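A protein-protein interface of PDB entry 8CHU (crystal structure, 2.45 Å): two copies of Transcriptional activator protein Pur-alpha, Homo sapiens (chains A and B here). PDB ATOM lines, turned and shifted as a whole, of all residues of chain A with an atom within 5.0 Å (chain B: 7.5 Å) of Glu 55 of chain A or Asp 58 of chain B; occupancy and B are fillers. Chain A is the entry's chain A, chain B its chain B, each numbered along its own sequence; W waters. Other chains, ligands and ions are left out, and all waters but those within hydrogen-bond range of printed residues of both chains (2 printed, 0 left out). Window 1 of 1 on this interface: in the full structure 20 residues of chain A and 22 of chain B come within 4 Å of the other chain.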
ATOM      1  N   SER A  51     -33.296 -27.107 -16.436  1.00  0.00           N
ATOM      2  CA  SER A  51     -32.763 -26.435 -15.229  1.00  0.00           C
ATOM      3  C   SER A  51     -32.359 -27.477 -14.192  1.00  0.00           C
ATOM      4  O   SER A  51     -31.264 -27.394 -13.631  1.00  0.00           O
ATOM      5  CB  SER A  51     -33.773 -25.510 -14.677  1.00  0.00           C
ATOM      6  OG  SER A  51     -33.845 -24.382 -15.521  1.00  0.00           O
ATOM      7  N   VAL A  52     -33.236 -28.438 -13.946  1.00  0.00           N
ATOM      8  CA  VAL A  52     -32.989 -29.521 -12.961  1.00  0.00           C
ATOM      9  C   VAL A  52     -31.958 -30.472 -13.568  1.00  0.00           C
ATOM     10  O   VAL A  52     -31.147 -30.997 -12.816  1.00  0.00           O
ATOM     11  CB  VAL A  52     -34.308 -30.228 -12.647  1.00  0.00           C
ATOM     12  CG1 VAL A  52     -34.091 -31.506 -11.845  1.00  0.00           C
ATOM     13  CG2 VAL A  52     -35.289 -29.271 -11.982  1.00  0.00           C
ATOM     14  N   ALA A  53     -31.961 -30.653 -14.894  1.00  0.00           N
ATOM     15  CA  ALA A  53     -30.956 -31.515 -15.551  1.00  0.00           C
ATOM     16  C   ALA A  53     -29.563 -31.000 -15.195  1.00  0.00           C
ATOM     17  O   ALA A  53     -28.676 -31.838 -14.931  1.00  0.00           O
ATOM     18  CB  ALA A  53     -31.158 -31.549 -17.038  1.00  0.00           C
ATOM     19  N   VAL A  54     -29.392 -29.674 -15.202  1.00  0.00           N
ATOM     20  CA  VAL A  54     -28.118 -28.939 -14.921  1.00  0.00           C
ATOM     21  C   VAL A  54     -27.715 -29.135 -13.459  1.00  0.00           C
ATOM     22  O   VAL A  54     -26.569 -29.481 -13.210  1.00  0.00           O
ATOM     23  CB  VAL A  54     -28.269 -27.448 -15.236  1.00  0.00           C
ATOM     24  CG1 VAL A  54     -27.138 -26.652 -14.613  1.00  0.00           C
ATOM     25  CG2 VAL A  54     -28.366 -27.198 -16.735  1.00  0.00           C
ATOM     26  N   GLU A  55     -28.668 -28.990 -12.549  1.00  0.00           N
ATOM     27  CA  GLU A  55     -28.523 -29.307 -11.100  1.00  0.00           C
ATOM     28  C   GLU A  55     -28.082 -30.762 -10.929  1.00  0.00           C
ATOM     29  O   GLU A  55     -27.114 -31.022 -10.166  1.00  0.00           O
ATOM     30  CB  GLU A  55     -29.836 -28.980 -10.381  1.00  0.00           C
ATOM     31  CG  GLU A  55     -30.117 -27.479 -10.304  1.00  0.00           C
ATOM     32  CD  GLU A  55     -31.561 -27.004 -10.285  1.00  0.00           C
ATOM     33  OE1 GLU A  55     -32.486 -27.851 -10.156  1.00  0.00           O
ATOM     34  OE2 GLU A  55     -31.753 -25.761 -10.369  1.00  0.00           O
ATOM     35  N   PHE A  56     -28.673 -31.654 -11.715  1.00  0.00           N
ATOM     36  CA  PHE A  56     -28.415 -33.115 -11.686  1.00  0.00           C
ATOM     37  C   PHE A  56     -26.982 -33.404 -12.141  1.00  0.00           C
ATOM     38  O   PHE A  56     -26.236 -34.147 -11.452  1.00  0.00           O
ATOM     39  CB  PHE A  56     -29.522 -33.826 -12.464  1.00  0.00           C
ATOM     40  CG  PHE A  56     -29.529 -35.319 -12.260  1.00  0.00           C
ATOM     41  CD1 PHE A  56     -29.623 -35.862 -10.983  1.00  0.00           C
ATOM     42  CD2 PHE A  56     -29.425 -36.179 -13.343  1.00  0.00           C
ATOM     43  CE1 PHE A  56     -29.584 -37.235 -10.794  1.00  0.00           C
ATOM     44  CE2 PHE A  56     -29.409 -37.552 -13.158  1.00  0.00           C
ATOM     45  CZ  PHE A  56     -29.474 -38.076 -11.885  1.00  0.00           C
ATOM     46  N   ARG A  57     -26.544 -32.760 -13.218  1.00  0.00           N
ATOM     47  CA  ARG A  57     -25.122 -32.776 -13.635  1.00  0.00           C
ATOM     48  C   ARG A  57     -24.200 -32.428 -12.459  1.00  0.00           C
ATOM     49  O   ARG A  57     -23.176 -33.109 -12.237  1.00  0.00           O
ATOM     50  CB  ARG A  57     -24.895 -31.741 -14.735  1.00  0.00           C
ATOM     51  CG  ARG A  57     -23.543 -31.874 -15.420  1.00  0.00           C
ATOM     52  CD  ARG A  57     -23.170 -30.638 -16.220  1.00  0.00           C
ATOM     53  NE  ARG A  57     -23.235 -29.441 -15.394  1.00  0.00           N
ATOM     54  CZ  ARG A  57     -23.561 -28.240 -15.836  1.00  0.00           C
ATOM     55  NH1 ARG A  57     -23.858 -28.036 -17.104  1.00  0.00           N
ATOM     56  NH2 ARG A  57     -23.617 -27.235 -14.992  1.00  0.00           N
ATOM     57  N   ASP A  58     -24.497 -31.358 -11.743  1.00  0.00           N
ATOM     58  CA  ASP A  58     -23.649 -30.921 -10.606  1.00  0.00           C
ATOM     59  C   ASP A  58     -23.693 -32.009  -9.506  1.00  0.00           C
ATOM     60  O   ASP A  58     -22.644 -32.357  -8.953  1.00  0.00           O
ATOM     61  CB  ASP A  58     -24.103 -29.554 -10.082  1.00  0.00           C
ATOM     62  CG  ASP A  58     -24.160 -28.442 -11.114  1.00  0.00           C
ATOM     63  OD1 ASP A  58     -23.326 -28.459 -12.044  1.00  0.00           O
ATOM     64  OD2 ASP A  58     -25.062 -27.567 -10.979  1.00  0.00           O
ATOM     65  N   TYR A  59     -24.869 -32.531  -9.168  1.00  0.00           N
ATOM     66  CA  TYR A  59     -24.970 -33.560  -8.112  1.00  0.00           C
ATOM     67  C   TYR A  59     -24.100 -34.738  -8.520  1.00  0.00           C
ATOM     68  O   TYR A  59     -23.400 -35.240  -7.658  1.00  0.00           O
ATOM     69  CB  TYR A  59     -26.425 -33.916  -7.791  1.00  0.00           C
ATOM     70  CG  TYR A  59     -27.280 -32.763  -7.291  1.00  0.00           C
ATOM     71  CD1 TYR A  59     -26.769 -31.754  -6.494  1.00  0.00           C
ATOM     72  CD2 TYR A  59     -28.617 -32.677  -7.634  1.00  0.00           C
ATOM     73  CE1 TYR A  59     -27.561 -30.701  -6.059  1.00  0.00           C
ATOM     74  CE2 TYR A  59     -29.416 -31.631  -7.226  1.00  0.00           C
ATOM     75  CZ  TYR A  59     -28.895 -30.643  -6.417  1.00  0.00           C
ATOM     76  OH  TYR A  59     -29.697 -29.605  -6.013  1.00  0.00           O
ATOM     77  N   LEU A  94     -33.883 -32.657  -3.230  1.00  0.00           N
ATOM     78  CA  LEU A  94     -34.265 -31.376  -3.868  1.00  0.00           C
ATOM     79  C   LEU A  94     -35.787 -31.346  -3.890  1.00  0.00           C
ATOM     80  O   LEU A  94     -36.413 -32.263  -4.446  1.00  0.00           O
ATOM     81  CB  LEU A  94     -33.690 -31.291  -5.283  1.00  0.00           C
ATOM     82  CG  LEU A  94     -34.301 -30.231  -6.197  1.00  0.00           C
ATOM     83  CD1 LEU A  94     -33.985 -28.819  -5.713  1.00  0.00           C
ATOM     84  CD2 LEU A  94     -33.826 -30.407  -7.623  1.00  0.00           C
ATOM     85  N   ARG A  96     -38.636 -29.100  -5.446  1.00  0.00           N
ATOM     86  CA  ARG A  96     -38.748 -28.016  -6.449  1.00  0.00           C
ATOM     87  C   ARG A  96     -40.149 -28.043  -6.999  1.00  0.00           C
ATOM     88  O   ARG A  96     -40.490 -29.080  -7.592  1.00  0.00           O
ATOM     89  CB  ARG A  96     -37.732 -28.194  -7.573  1.00  0.00           C
ATOM     90  CG  ARG A  96     -37.690 -27.033  -8.548  1.00  0.00           C
ATOM     91  CD  ARG A  96     -36.595 -27.315  -9.554  1.00  0.00           C
ATOM     92  NE  ARG A  96     -36.655 -26.412 -10.696  1.00  0.00           N
ATOM     93  CZ  ARG A  96     -37.563 -26.455 -11.675  1.00  0.00           C
ATOM     94  NH1 ARG A  96     -38.487 -27.405 -11.700  1.00  0.00           N
ATOM     95  NH2 ARG A  96     -37.524 -25.548 -12.640  1.00  0.00           N
ATOM     96  N   GLU A 158     -30.343 -22.171 -19.364  1.00  0.00           N
ATOM     97  CA  GLU A 158     -29.957 -21.728 -17.973  1.00  0.00           C
ATOM     98  C   GLU A 158     -29.428 -20.273 -17.930  1.00  0.00           C
ATOM     99  O   GLU A 158     -30.068 -19.336 -17.396  1.00  0.00           O
ATOM    100  CB  GLU A 158     -28.944 -22.706 -17.353  1.00  0.00           C
ATOM    101  CG  GLU A 158     -28.973 -22.803 -15.822  1.00  0.00           C
ATOM    102  CD  GLU A 158     -30.077 -23.682 -15.230  1.00  0.00           C
ATOM    103  OE1 GLU A 158     -31.223 -23.556 -15.734  1.00  0.00           O
ATOM    104  OE2 GLU A 158     -29.809 -24.498 -14.254  1.00  0.00           O
ATOM    105  OXT GLU A 158     -28.326 -19.924 -18.380  1.00  0.00           O
ATOM    106  N   SER B  51     -17.924 -26.609  -4.588  1.00  0.00           N
ATOM    107  CA  SER B  51     -18.986 -27.464  -5.183  1.00  0.00           C
ATOM    108  C   SER B  51     -20.384 -26.904  -4.875  1.00  0.00           C
ATOM    109  O   SER B  51     -21.241 -26.881  -5.818  1.00  0.00           O
ATOM    110  CB  SER B  51     -18.857 -28.903  -4.777  1.00  0.00           C
ATOM    111  OG  SER B  51     -18.313 -28.977  -3.483  1.00  0.00           O
ATOM    112  N   VAL B  52     -20.644 -26.432  -3.657  1.00  0.00           N
ATOM    113  CA  VAL B  52     -21.968 -25.789  -3.391  1.00  0.00           C
ATOM    114  C   VAL B  52     -22.145 -24.522  -4.244  1.00  0.00           C
ATOM    115  O   VAL B  52     -23.294 -24.277  -4.656  1.00  0.00           O
ATOM    116  CB  VAL B  52     -22.192 -25.516  -1.904  1.00  0.00           C
ATOM    117  CG1 VAL B  52     -23.450 -24.681  -1.679  1.00  0.00           C
ATOM    118  CG2 VAL B  52     -22.276 -26.834  -1.158  1.00  0.00           C
ATOM    119  N   ALA B  53     -21.071 -23.783  -4.541  1.00  0.00           N
ATOM    120  CA  ALA B  53     -21.088 -22.577  -5.410  1.00  0.00           C
ATOM    121  C   ALA B  53     -21.499 -22.923  -6.849  1.00  0.00           C
ATOM    122  O   ALA B  53     -22.267 -22.154  -7.481  1.00  0.00           O
ATOM    123  CB  ALA B  53     -19.728 -21.919  -5.423  1.00  0.00           C
ATOM    124  N   VAL B  54     -20.920 -23.974  -7.411  1.00  0.00           N
ATOM    125  CA  VAL B  54     -21.361 -24.510  -8.725  1.00  0.00           C
ATOM    126  C   VAL B  54     -22.872 -24.737  -8.646  1.00  0.00           C
ATOM    127  O   VAL B  54     -23.637 -24.221  -9.486  1.00  0.00           O
ATOM    128  CB  VAL B  54     -20.568 -25.799  -9.015  1.00  0.00           C
ATOM    129  CG1 VAL B  54     -21.209 -26.641 -10.120  1.00  0.00           C
ATOM    130  CG2 VAL B  54     -19.117 -25.474  -9.345  1.00  0.00           C
ATOM    131  N   GLU B  55     -23.321 -25.419  -7.603  1.00  0.00           N
ATOM    132  CA  GLU B  55     -24.756 -25.748  -7.455  1.00  0.00           C
ATOM    133  C   GLU B  55     -25.538 -24.448  -7.435  1.00  0.00           C
ATOM    134  O   GLU B  55     -26.587 -24.376  -8.070  1.00  0.00           O
ATOM    135  CB  GLU B  55     -25.006 -26.577  -6.201  1.00  0.00           C
ATOM    136  CG  GLU B  55     -25.065 -28.067  -6.478  1.00  0.00           C
ATOM    137  CD  GLU B  55     -24.154 -28.968  -5.666  1.00  0.00           C
ATOM    138  OE1 GLU B  55     -24.201 -28.917  -4.428  1.00  0.00           O
ATOM    139  OE2 GLU B  55     -23.441 -29.747  -6.303  1.00  0.00           O
ATOM    140  N   PHE B  56     -25.031 -23.483  -6.683  1.00  0.00           N
ATOM    141  CA  PHE B  56     -25.726 -22.221  -6.357  1.00  0.00           C
ATOM    142  C   PHE B  56     -25.824 -21.371  -7.621  1.00  0.00           C
ATOM    143  O   PHE B  56     -26.866 -20.772  -7.916  1.00  0.00           O
ATOM    144  CB  PHE B  56     -24.950 -21.494  -5.264  1.00  0.00           C
ATOM    145  CG  PHE B  56     -25.495 -20.134  -4.940  1.00  0.00           C
ATOM    146  CD1 PHE B  56     -26.844 -19.964  -4.671  1.00  0.00           C
ATOM    147  CD2 PHE B  56     -24.660 -19.034  -4.885  1.00  0.00           C
ATOM    148  CE1 PHE B  56     -27.346 -18.717  -4.348  1.00  0.00           C
ATOM    149  CE2 PHE B  56     -25.163 -17.796  -4.535  1.00  0.00           C
ATOM    150  CZ  PHE B  56     -26.499 -17.642  -4.265  1.00  0.00           C
ATOM    151  N   ARG B  57     -24.740 -21.328  -8.378  1.00  0.00           N
ATOM    152  CA  ARG B  57     -24.763 -20.707  -9.725  1.00  0.00           C
ATOM    153  C   ARG B  57     -25.971 -21.248 -10.510  1.00  0.00           C
ATOM    154  O   ARG B  57     -26.707 -20.451 -11.126  1.00  0.00           O
ATOM    155  CB  ARG B  57     -23.456 -21.025 -10.426  1.00  0.00           C
ATOM    156  CG  ARG B  57     -23.452 -20.571 -11.866  1.00  0.00           C
ATOM    157  CD  ARG B  57     -22.294 -21.261 -12.509  1.00  0.00           C
ATOM    158  NE  ARG B  57     -22.634 -22.659 -12.670  1.00  0.00           N
ATOM    159  CZ  ARG B  57     -21.755 -23.578 -13.023  1.00  0.00           C
ATOM    160  NH1 ARG B  57     -20.486 -23.212 -13.201  1.00  0.00           N
ATOM    161  NH2 ARG B  57     -22.148 -24.841 -13.149  1.00  0.00           N
ATOM    162  N   ASP B  58     -26.185 -22.564 -10.474  1.00  0.00           N
ATOM    163  CA  ASP B  58     -27.245 -23.213 -11.279  1.00  0.00           C
ATOM    164  C   ASP B  58     -28.619 -23.003 -10.637  1.00  0.00           C
ATOM    165  O   ASP B  58     -29.560 -22.745 -11.386  1.00  0.00           O
ATOM    166  CB  ASP B  58     -26.866 -24.662 -11.518  1.00  0.00           C
ATOM    167  CG  ASP B  58     -25.628 -24.774 -12.385  1.00  0.00           C
ATOM    168  OD1 ASP B  58     -25.380 -23.891 -13.240  1.00  0.00           O
ATOM    169  OD2 ASP B  58     -24.911 -25.708 -12.161  1.00  0.00           O
ATOM    170  N   TYR B  59     -28.761 -23.049  -9.313  1.00  0.00           N
ATOM    171  CA  TYR B  59     -30.031 -22.631  -8.672  1.00  0.00           C
ATOM    172  C   TYR B  59     -30.390 -21.228  -9.176  1.00  0.00           C
ATOM    173  O   TYR B  59     -31.544 -21.043  -9.596  1.00  0.00           O
ATOM    174  CB  TYR B  59     -29.971 -22.712  -7.146  1.00  0.00           C
ATOM    175  CG  TYR B  59     -29.543 -24.040  -6.582  1.00  0.00           C
ATOM    176  CD1 TYR B  59     -29.767 -25.242  -7.247  1.00  0.00           C
ATOM    177  CD2 TYR B  59     -28.901 -24.097  -5.357  1.00  0.00           C
ATOM    178  CE1 TYR B  59     -29.342 -26.454  -6.713  1.00  0.00           C
ATOM    179  CE2 TYR B  59     -28.508 -25.303  -4.792  1.00  0.00           C
ATOM    180  CZ  TYR B  59     -28.709 -26.487  -5.481  1.00  0.00           C
ATOM    181  OH  TYR B  59     -28.301 -27.654  -4.898  1.00  0.00           O
ATOM    182  N   LEU B  60     -29.454 -20.271  -9.189  1.00  0.00           N
ATOM    183  CA  LEU B  60     -29.768 -18.895  -9.670  1.00  0.00           C
ATOM    184  C   LEU B  60     -30.235 -19.008 -11.128  1.00  0.00           C
ATOM    185  O   LEU B  60     -31.218 -18.343 -11.515  1.00  0.00           O
ATOM    186  CB  LEU B  60     -28.555 -17.960  -9.544  1.00  0.00           C
ATOM    187  CG  LEU B  60     -28.112 -17.591  -8.118  1.00  0.00           C
ATOM    188  CD1 LEU B  60     -26.882 -16.704  -8.140  1.00  0.00           C
ATOM    189  CD2 LEU B  60     -29.214 -16.922  -7.322  1.00  0.00           C
ATOM    190  N   GLY B  61     -29.535 -19.817 -11.913  1.00  0.00           N
ATOM    191  CA  GLY B  61     -29.887 -20.064 -13.324  1.00  0.00           C
ATOM    192  C   GLY B  61     -31.326 -20.539 -13.488  1.00  0.00           C
ATOM    193  O   GLY B  61     -32.023 -20.038 -14.361  1.00  0.00           O
ATOM    194  N   ASP B  62     -31.745 -21.455 -12.632  1.00  0.00           N
ATOM    195  CA  ASP B  62     -33.105 -22.040 -12.563  1.00  0.00           C
ATOM    196  C   ASP B  62     -34.134 -20.919 -12.346  1.00  0.00           C
ATOM    197  O   ASP B  62     -35.089 -20.844 -13.136  1.00  0.00           O
ATOM    198  CB  ASP B  62     -33.112 -23.140 -11.500  1.00  0.00           C
ATOM    199  CG  ASP B  62     -34.341 -24.012 -11.550  1.00  0.00           C
ATOM    200  OD1 ASP B  62     -35.289 -23.587 -12.210  1.00  0.00           O
ATOM    201  OD2 ASP B  62     -34.334 -25.100 -10.923  1.00  0.00           O
ATOM    202  N   PHE B  63     -33.926 -20.061 -11.346  1.00  0.00           N
ATOM    203  CA  PHE B  63     -34.823 -18.921 -11.016  1.00  0.00           C
ATOM    204  C   PHE B  63     -34.842 -17.904 -12.162  1.00  0.00           C
ATOM    205  O   PHE B  63     -35.922 -17.422 -12.539  1.00  0.00           O
ATOM    206  CB  PHE B  63     -34.379 -18.258  -9.710  1.00  0.00           C
ATOM    207  CG  PHE B  63     -34.945 -18.937  -8.496  1.00  0.00           C
ATOM    208  CD1 PHE B  63     -36.187 -18.582  -8.012  1.00  0.00           C
ATOM    209  CD2 PHE B  63     -34.290 -19.995  -7.905  1.00  0.00           C
ATOM    210  CE1 PHE B  63     -36.736 -19.225  -6.918  1.00  0.00           C
ATOM    211  CE2 PHE B  63     -34.830 -20.635  -6.808  1.00  0.00           C
ATOM    212  CZ  PHE B  63     -36.051 -20.247  -6.317  1.00  0.00           C
ATOM    213  N   ILE B  64     -33.678 -17.602 -12.732  1.00  0.00           N
ATOM    214  CA  ILE B  64     -33.607 -16.689 -13.894  1.00  0.00           C
ATOM    215  C   ILE B  64     -34.502 -17.278 -14.989  1.00  0.00           C
ATOM    216  O   ILE B  64     -35.320 -16.544 -15.535  1.00  0.00           O
ATOM    217  CB  ILE B  64     -32.156 -16.446 -14.353  1.00  0.00           C
ATOM    218  CG1 ILE B  64     -31.340 -15.751 -13.259  1.00  0.00           C
ATOM    219  CG2 ILE B  64     -32.140 -15.647 -15.667  1.00  0.00           C
ATOM    220  CD1 ILE B  64     -29.821 -15.830 -13.447  1.00  0.00           C
ATOM    221  N   GLU B  65     -34.418 -18.578 -15.251  1.00  0.00           N
ATOM    222  CA  GLU B  65     -35.241 -19.204 -16.312  1.00  0.00           C
ATOM    223  C   GLU B  65     -36.712 -19.263 -15.880  1.00  0.00           C
ATOM    224  O   GLU B  65     -37.587 -19.272 -16.761  1.00  0.00           O
ATOM    225  CB  GLU B  65     -34.667 -20.575 -16.690  1.00  0.00           C
ATOM    226  CG  GLU B  65     -33.504 -20.475 -17.662  1.00  0.00           C
ATOM    227  CD  GLU B  65     -33.906 -20.088 -19.077  1.00  0.00           C
ATOM    228  OE1 GLU B  65     -34.669 -20.866 -19.706  1.00  0.00           O
ATOM    229  OE2 GLU B  65     -33.459 -19.020 -19.559  1.00  0.00           O
ATOM    230  N   HIS B  66     -37.001 -19.311 -14.579  1.00  0.00           N
ATOM    231  CA  HIS B  66     -38.305 -19.822 -14.076  1.00  0.00           C
ATOM    232  C   HIS B  66     -38.835 -18.954 -12.937  1.00  0.00           C
ATOM    233  O   HIS B  66     -39.518 -19.510 -12.052  1.00  0.00           O
ATOM    234  CB  HIS B  66     -38.170 -21.286 -13.634  1.00  0.00           C
ATOM    235  CG  HIS B  66     -37.909 -22.217 -14.761  1.00  0.00           C
ATOM    236  ND1 HIS B  66     -36.856 -23.089 -14.760  1.00  0.00           N
ATOM    237  CD2 HIS B  66     -38.545 -22.397 -15.932  1.00  0.00           C
ATOM    238  CE1 HIS B  66     -36.863 -23.779 -15.879  1.00  0.00           C
ATOM    239  NE2 HIS B  66     -37.883 -23.371 -16.610  1.00  0.00           N
ATOM    240  N   LEU B  70     -41.578 -20.268 -10.108  1.00  0.00           N
ATOM    241  CA  LEU B  70     -40.926 -20.653  -8.826  1.00  0.00           C
ATOM    242  C   LEU B  70     -41.300 -19.676  -7.702  1.00  0.00           C
ATOM    243  O   LEU B  70     -40.975 -20.001  -6.529  1.00  0.00           O
ATOM    244  CB  LEU B  70     -39.408 -20.694  -9.015  1.00  0.00           C
ATOM    245  CG  LEU B  70     -38.843 -22.030  -9.490  1.00  0.00           C
ATOM    246  CD1 LEU B  70     -37.401 -21.869  -9.905  1.00  0.00           C
ATOM    247  CD2 LEU B  70     -38.975 -23.089  -8.411  1.00  0.00           C
ATOM    248  N   PHE B  93     -38.381 -24.345  -2.639  1.00  0.00           N
ATOM    249  CA  PHE B  93     -37.118 -24.689  -3.330  1.00  0.00           C
ATOM    250  C   PHE B  93     -36.094 -24.945  -2.254  1.00  0.00           C
ATOM    251  O   PHE B  93     -35.589 -23.951  -1.725  1.00  0.00           O
ATOM    252  CB  PHE B  93     -36.611 -23.598  -4.276  1.00  0.00           C
ATOM    253  CG  PHE B  93     -35.484 -24.093  -5.144  1.00  0.00           C
ATOM    254  CD1 PHE B  93     -34.296 -24.550  -4.578  1.00  0.00           C
ATOM    255  CD2 PHE B  93     -35.630 -24.173  -6.521  1.00  0.00           C
ATOM    256  CE1 PHE B  93     -33.275 -25.049  -5.378  1.00  0.00           C
ATOM    257  CE2 PHE B  93     -34.611 -24.681  -7.315  1.00  0.00           C
ATOM    258  CZ  PHE B  93     -33.435 -25.115  -6.743  1.00  0.00           C
ATOM    259  N   VAL B  95     -32.784 -27.696  -0.807  1.00  0.00           N
ATOM    260  CA  VAL B  95     -31.763 -28.726  -1.122  1.00  0.00           C
ATOM    261  C   VAL B  95     -31.234 -29.196   0.225  1.00  0.00           C
ATOM    262  O   VAL B  95     -30.948 -28.348   1.048  1.00  0.00           O
ATOM    263  CB  VAL B  95     -30.645 -28.175  -2.036  1.00  0.00           C
ATOM    264  CG1 VAL B  95     -29.636 -29.245  -2.404  1.00  0.00           C
ATOM    265  CG2 VAL B  95     -31.195 -27.559  -3.306  1.00  0.00           C
ATOM    266  N   LEU B 105     -34.177 -21.328  -0.993  1.00  0.00           N
ATOM    267  CA  LEU B 105     -34.248 -20.126  -1.853  1.00  0.00           C
ATOM    268  C   LEU B 105     -35.718 -19.812  -2.003  1.00  0.00           C
ATOM    269  O   LEU B 105     -36.437 -20.781  -2.306  1.00  0.00           O
ATOM    270  CB  LEU B 105     -33.670 -20.433  -3.227  1.00  0.00           C
ATOM    271  CG  LEU B 105     -32.152 -20.516  -3.334  1.00  0.00           C
ATOM    272  CD1 LEU B 105     -31.650 -21.930  -3.000  1.00  0.00           C
ATOM    273  CD2 LEU B 105     -31.741 -20.110  -4.747  1.00  0.00           C
ATOM    274  N   ARG B 145     -25.210 -13.629 -10.960  1.00  0.00           N
ATOM    275  CA  ARG B 145     -24.944 -15.005 -11.403  1.00  0.00           C
ATOM    276  C   ARG B 145     -23.777 -15.005 -12.384  1.00  0.00           C
ATOM    277  O   ARG B 145     -22.943 -15.935 -12.285  1.00  0.00           O
ATOM    278  CB  ARG B 145     -26.193 -15.605 -12.029  1.00  0.00           C
ATOM    279  CG  ARG B 145     -26.014 -17.063 -12.399  1.00  0.00           C
ATOM    280  CD  ARG B 145     -25.639 -17.268 -13.835  1.00  0.00           C
ATOM    281  NE  ARG B 145     -25.643 -18.714 -13.965  1.00  0.00           N
ATOM    282  CZ  ARG B 145     -26.430 -19.412 -14.759  1.00  0.00           C
ATOM    283  NH1 ARG B 145     -27.266 -18.777 -15.567  1.00  0.00           N
ATOM    284  NH2 ARG B 145     -26.350 -20.742 -14.753  1.00  0.00           N
ATOM    285  N   LEU B 148     -20.689 -14.623 -10.361  1.00  0.00           N
ATOM    286  CA  LEU B 148     -20.420 -15.885  -9.636  1.00  0.00           C
ATOM    287  C   LEU B 148     -19.778 -16.872 -10.622  1.00  0.00           C
ATOM    288  O   LEU B 148     -18.724 -17.460 -10.291  1.00  0.00           O
ATOM    289  CB  LEU B 148     -21.745 -16.379  -9.060  1.00  0.00           C
ATOM    290  CG  LEU B 148     -21.721 -17.784  -8.490  1.00  0.00           C
ATOM    291  CD1 LEU B 148     -20.630 -17.928  -7.466  1.00  0.00           C
ATOM    292  CD2 LEU B 148     -23.051 -18.133  -7.868  1.00  0.00           C
ATOM    293  N   ILE B 152     -16.036 -18.982 -10.727  1.00  0.00           N
ATOM    294  CA  ILE B 152     -15.922 -20.465 -10.804  1.00  0.00           C
ATOM    295  C   ILE B 152     -15.045 -20.858 -12.009  1.00  0.00           C
ATOM    296  O   ILE B 152     -14.131 -21.676 -11.812  1.00  0.00           O
ATOM    297  CB  ILE B 152     -17.322 -21.119 -10.798  1.00  0.00           C
ATOM    298  CG1 ILE B 152     -18.028 -20.850  -9.458  1.00  0.00           C
ATOM    299  CG2 ILE B 152     -17.193 -22.604 -11.095  1.00  0.00           C
ATOM    300  CD1 ILE B 152     -19.528 -20.937  -9.495  1.00  0.00           C
HETATM  301  O   HOH W   1     -35.776 -25.699 -17.864  1.00  0.00           O
HETATM  302  O   HOH W   2     -24.233 -24.634 -15.789  1.00  0.00           O
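Water W2 lies within hydrogen-bond range of the guanidinium group of Arg 57 of chain A (2.8 Å), the side-chain carboxylate of Asp 58 of chain B (2.9 Å) and the guanidinium group of Arg 57 of chain B (3.4 Å).
Water W1 lies within hydrogen-bond range of N of Ser 51 of chain A and NE2 of His 66 of chain B.
Of chain B, only Asp 58, Tyr 59 and Asp 62 come within 4 Å of Glu 55 of chain A.
Printed residues of chain B within 4 Å of Tyr 59 of chain A: Glu 55, Tyr 59 and Val 95.
Printed residues of chain B within 4 Å of Leu 94 of chain A: Phe 93 (3.9 Å) and Val 95 (3.9 Å).
Asp 58 of chain B touches just these residues of chain A: Val 54, Glu 55, Arg 57, Asp 58 and Glu 158.
Ile 64 of chain B touches none of the printed residues of chain A.
Printed residues of chain A within 4 Å of Glu 65 of chain B: Glu 158 (3.6 Å).
Leu 148 of chain B touches none of the printed residues of chain A.
The nearest printed residue of chain A that does not touch Asp 58 of chain B is Ser 51 of chain A (5.4 Å).
The side-chain carboxylate (OE1) of Glu 158 of chain A is in hydrogen-bond range of the side-chain hydroxyl (OG) of Ser 51 of chain A, at 2.8 Å.
The guanidinium group (NH2) of Arg 57 of chain B lies within salt-bridge range of the side-chain carboxylate (OD2) of Asp 58 of chain B (3.1 Å).
ND1 of His 66 of chain B is in hydrogen-bond range of OD1 of Asp 62 of chain B (3.0 Å).
The side-chain carboxylate of Asp 58 of chain B lies within salt-bridge range of the guanidinium group of Arg 57 of chain A (3.5 Å).
OE2 of Glu 158 of chain A sits close to O of Asp 58 of chain B, 3.4 Å away.
OH of Tyr 59 of chain A is in hydrogen-bond range of OH of Tyr 59 of chain B, at 2.6 Å.
NH2 of Arg 57 of chain A lies close to NH2 of Arg 57 of chain B (3.4 Å).
The guanidinium group of Arg 96 of chain A lies within hydrogen-bond range of a ring nitrogen (ND1) of His 66 of chain B, at 3.3 Å.
The side-chain hydroxyl (OG) of Ser 51 of chain A lies close to a ring nitrogen (ND1) of His 66 of chain B (3.4 Å).
The chain-end carboxylate of Glu 158 of chain A lies within salt-bridge range of the guanidinium group of Arg 145 of chain B (3.2 Å).
NE of Arg 96 of chain A is in salt-bridge range of OD2 of Asp 62 of chain B, 2.7 Å away.
The side-chain carboxylate (OD2) of Asp 58 of chain A lies close to the side-chain carboxylate (OD2) of Asp 58 of chain B, 2.2 Å away.
OE2 of Glu 55 of chain A lies close to OD2 of Asp 62 of chain B (2.7 Å).
The side-chain carboxylate of Asp 58 of chain A lies within salt-bridge range of the guanidinium group of Arg 57 of chain B, at 3.96 Å.
Of the 12 printed residues of chain A, 9 touch a printed residue of chain B.
Hydrophobic or aromatic side chains of chain A within 4 Å of the printed part of chain B: Val 54, Tyr 59 and Leu 94.
Val 54 of chain A touches Asp 58 of chain B, and with the chains exchanged Asp 58 of chain A touches Val 54 of chain B.
Glu 55 of chain A touches Tyr 59 of chain B, and with the chains exchanged Tyr 59 of chain A touches Glu 55 of chain B.
Arg 57 of chain A touches its own counterpart, Arg 57 of chain B.
Asp 58 of chain A touches its own counterpart, Asp 58 of chain B.
Val 54 of chain A touches Asp 58 of chain B.
Glu 55 of chain B touches Asp 58 of chain A.
Glu 55 of chain B touches Tyr 59 of chain A.
Tyr 59 of chain A touches Val 95 of chain B.
Val 95 of chain B touches Leu 94 of chain A.
Arg 96 of chain A touches Phe 93 of chain B (CD to CE2, 3.99 Å).
Glu 158 of chain A touches Asp 62 of chain B (OE1 to N, 3.8 Å).
Glu 158 of chain A touches Glu 65 of chain B.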
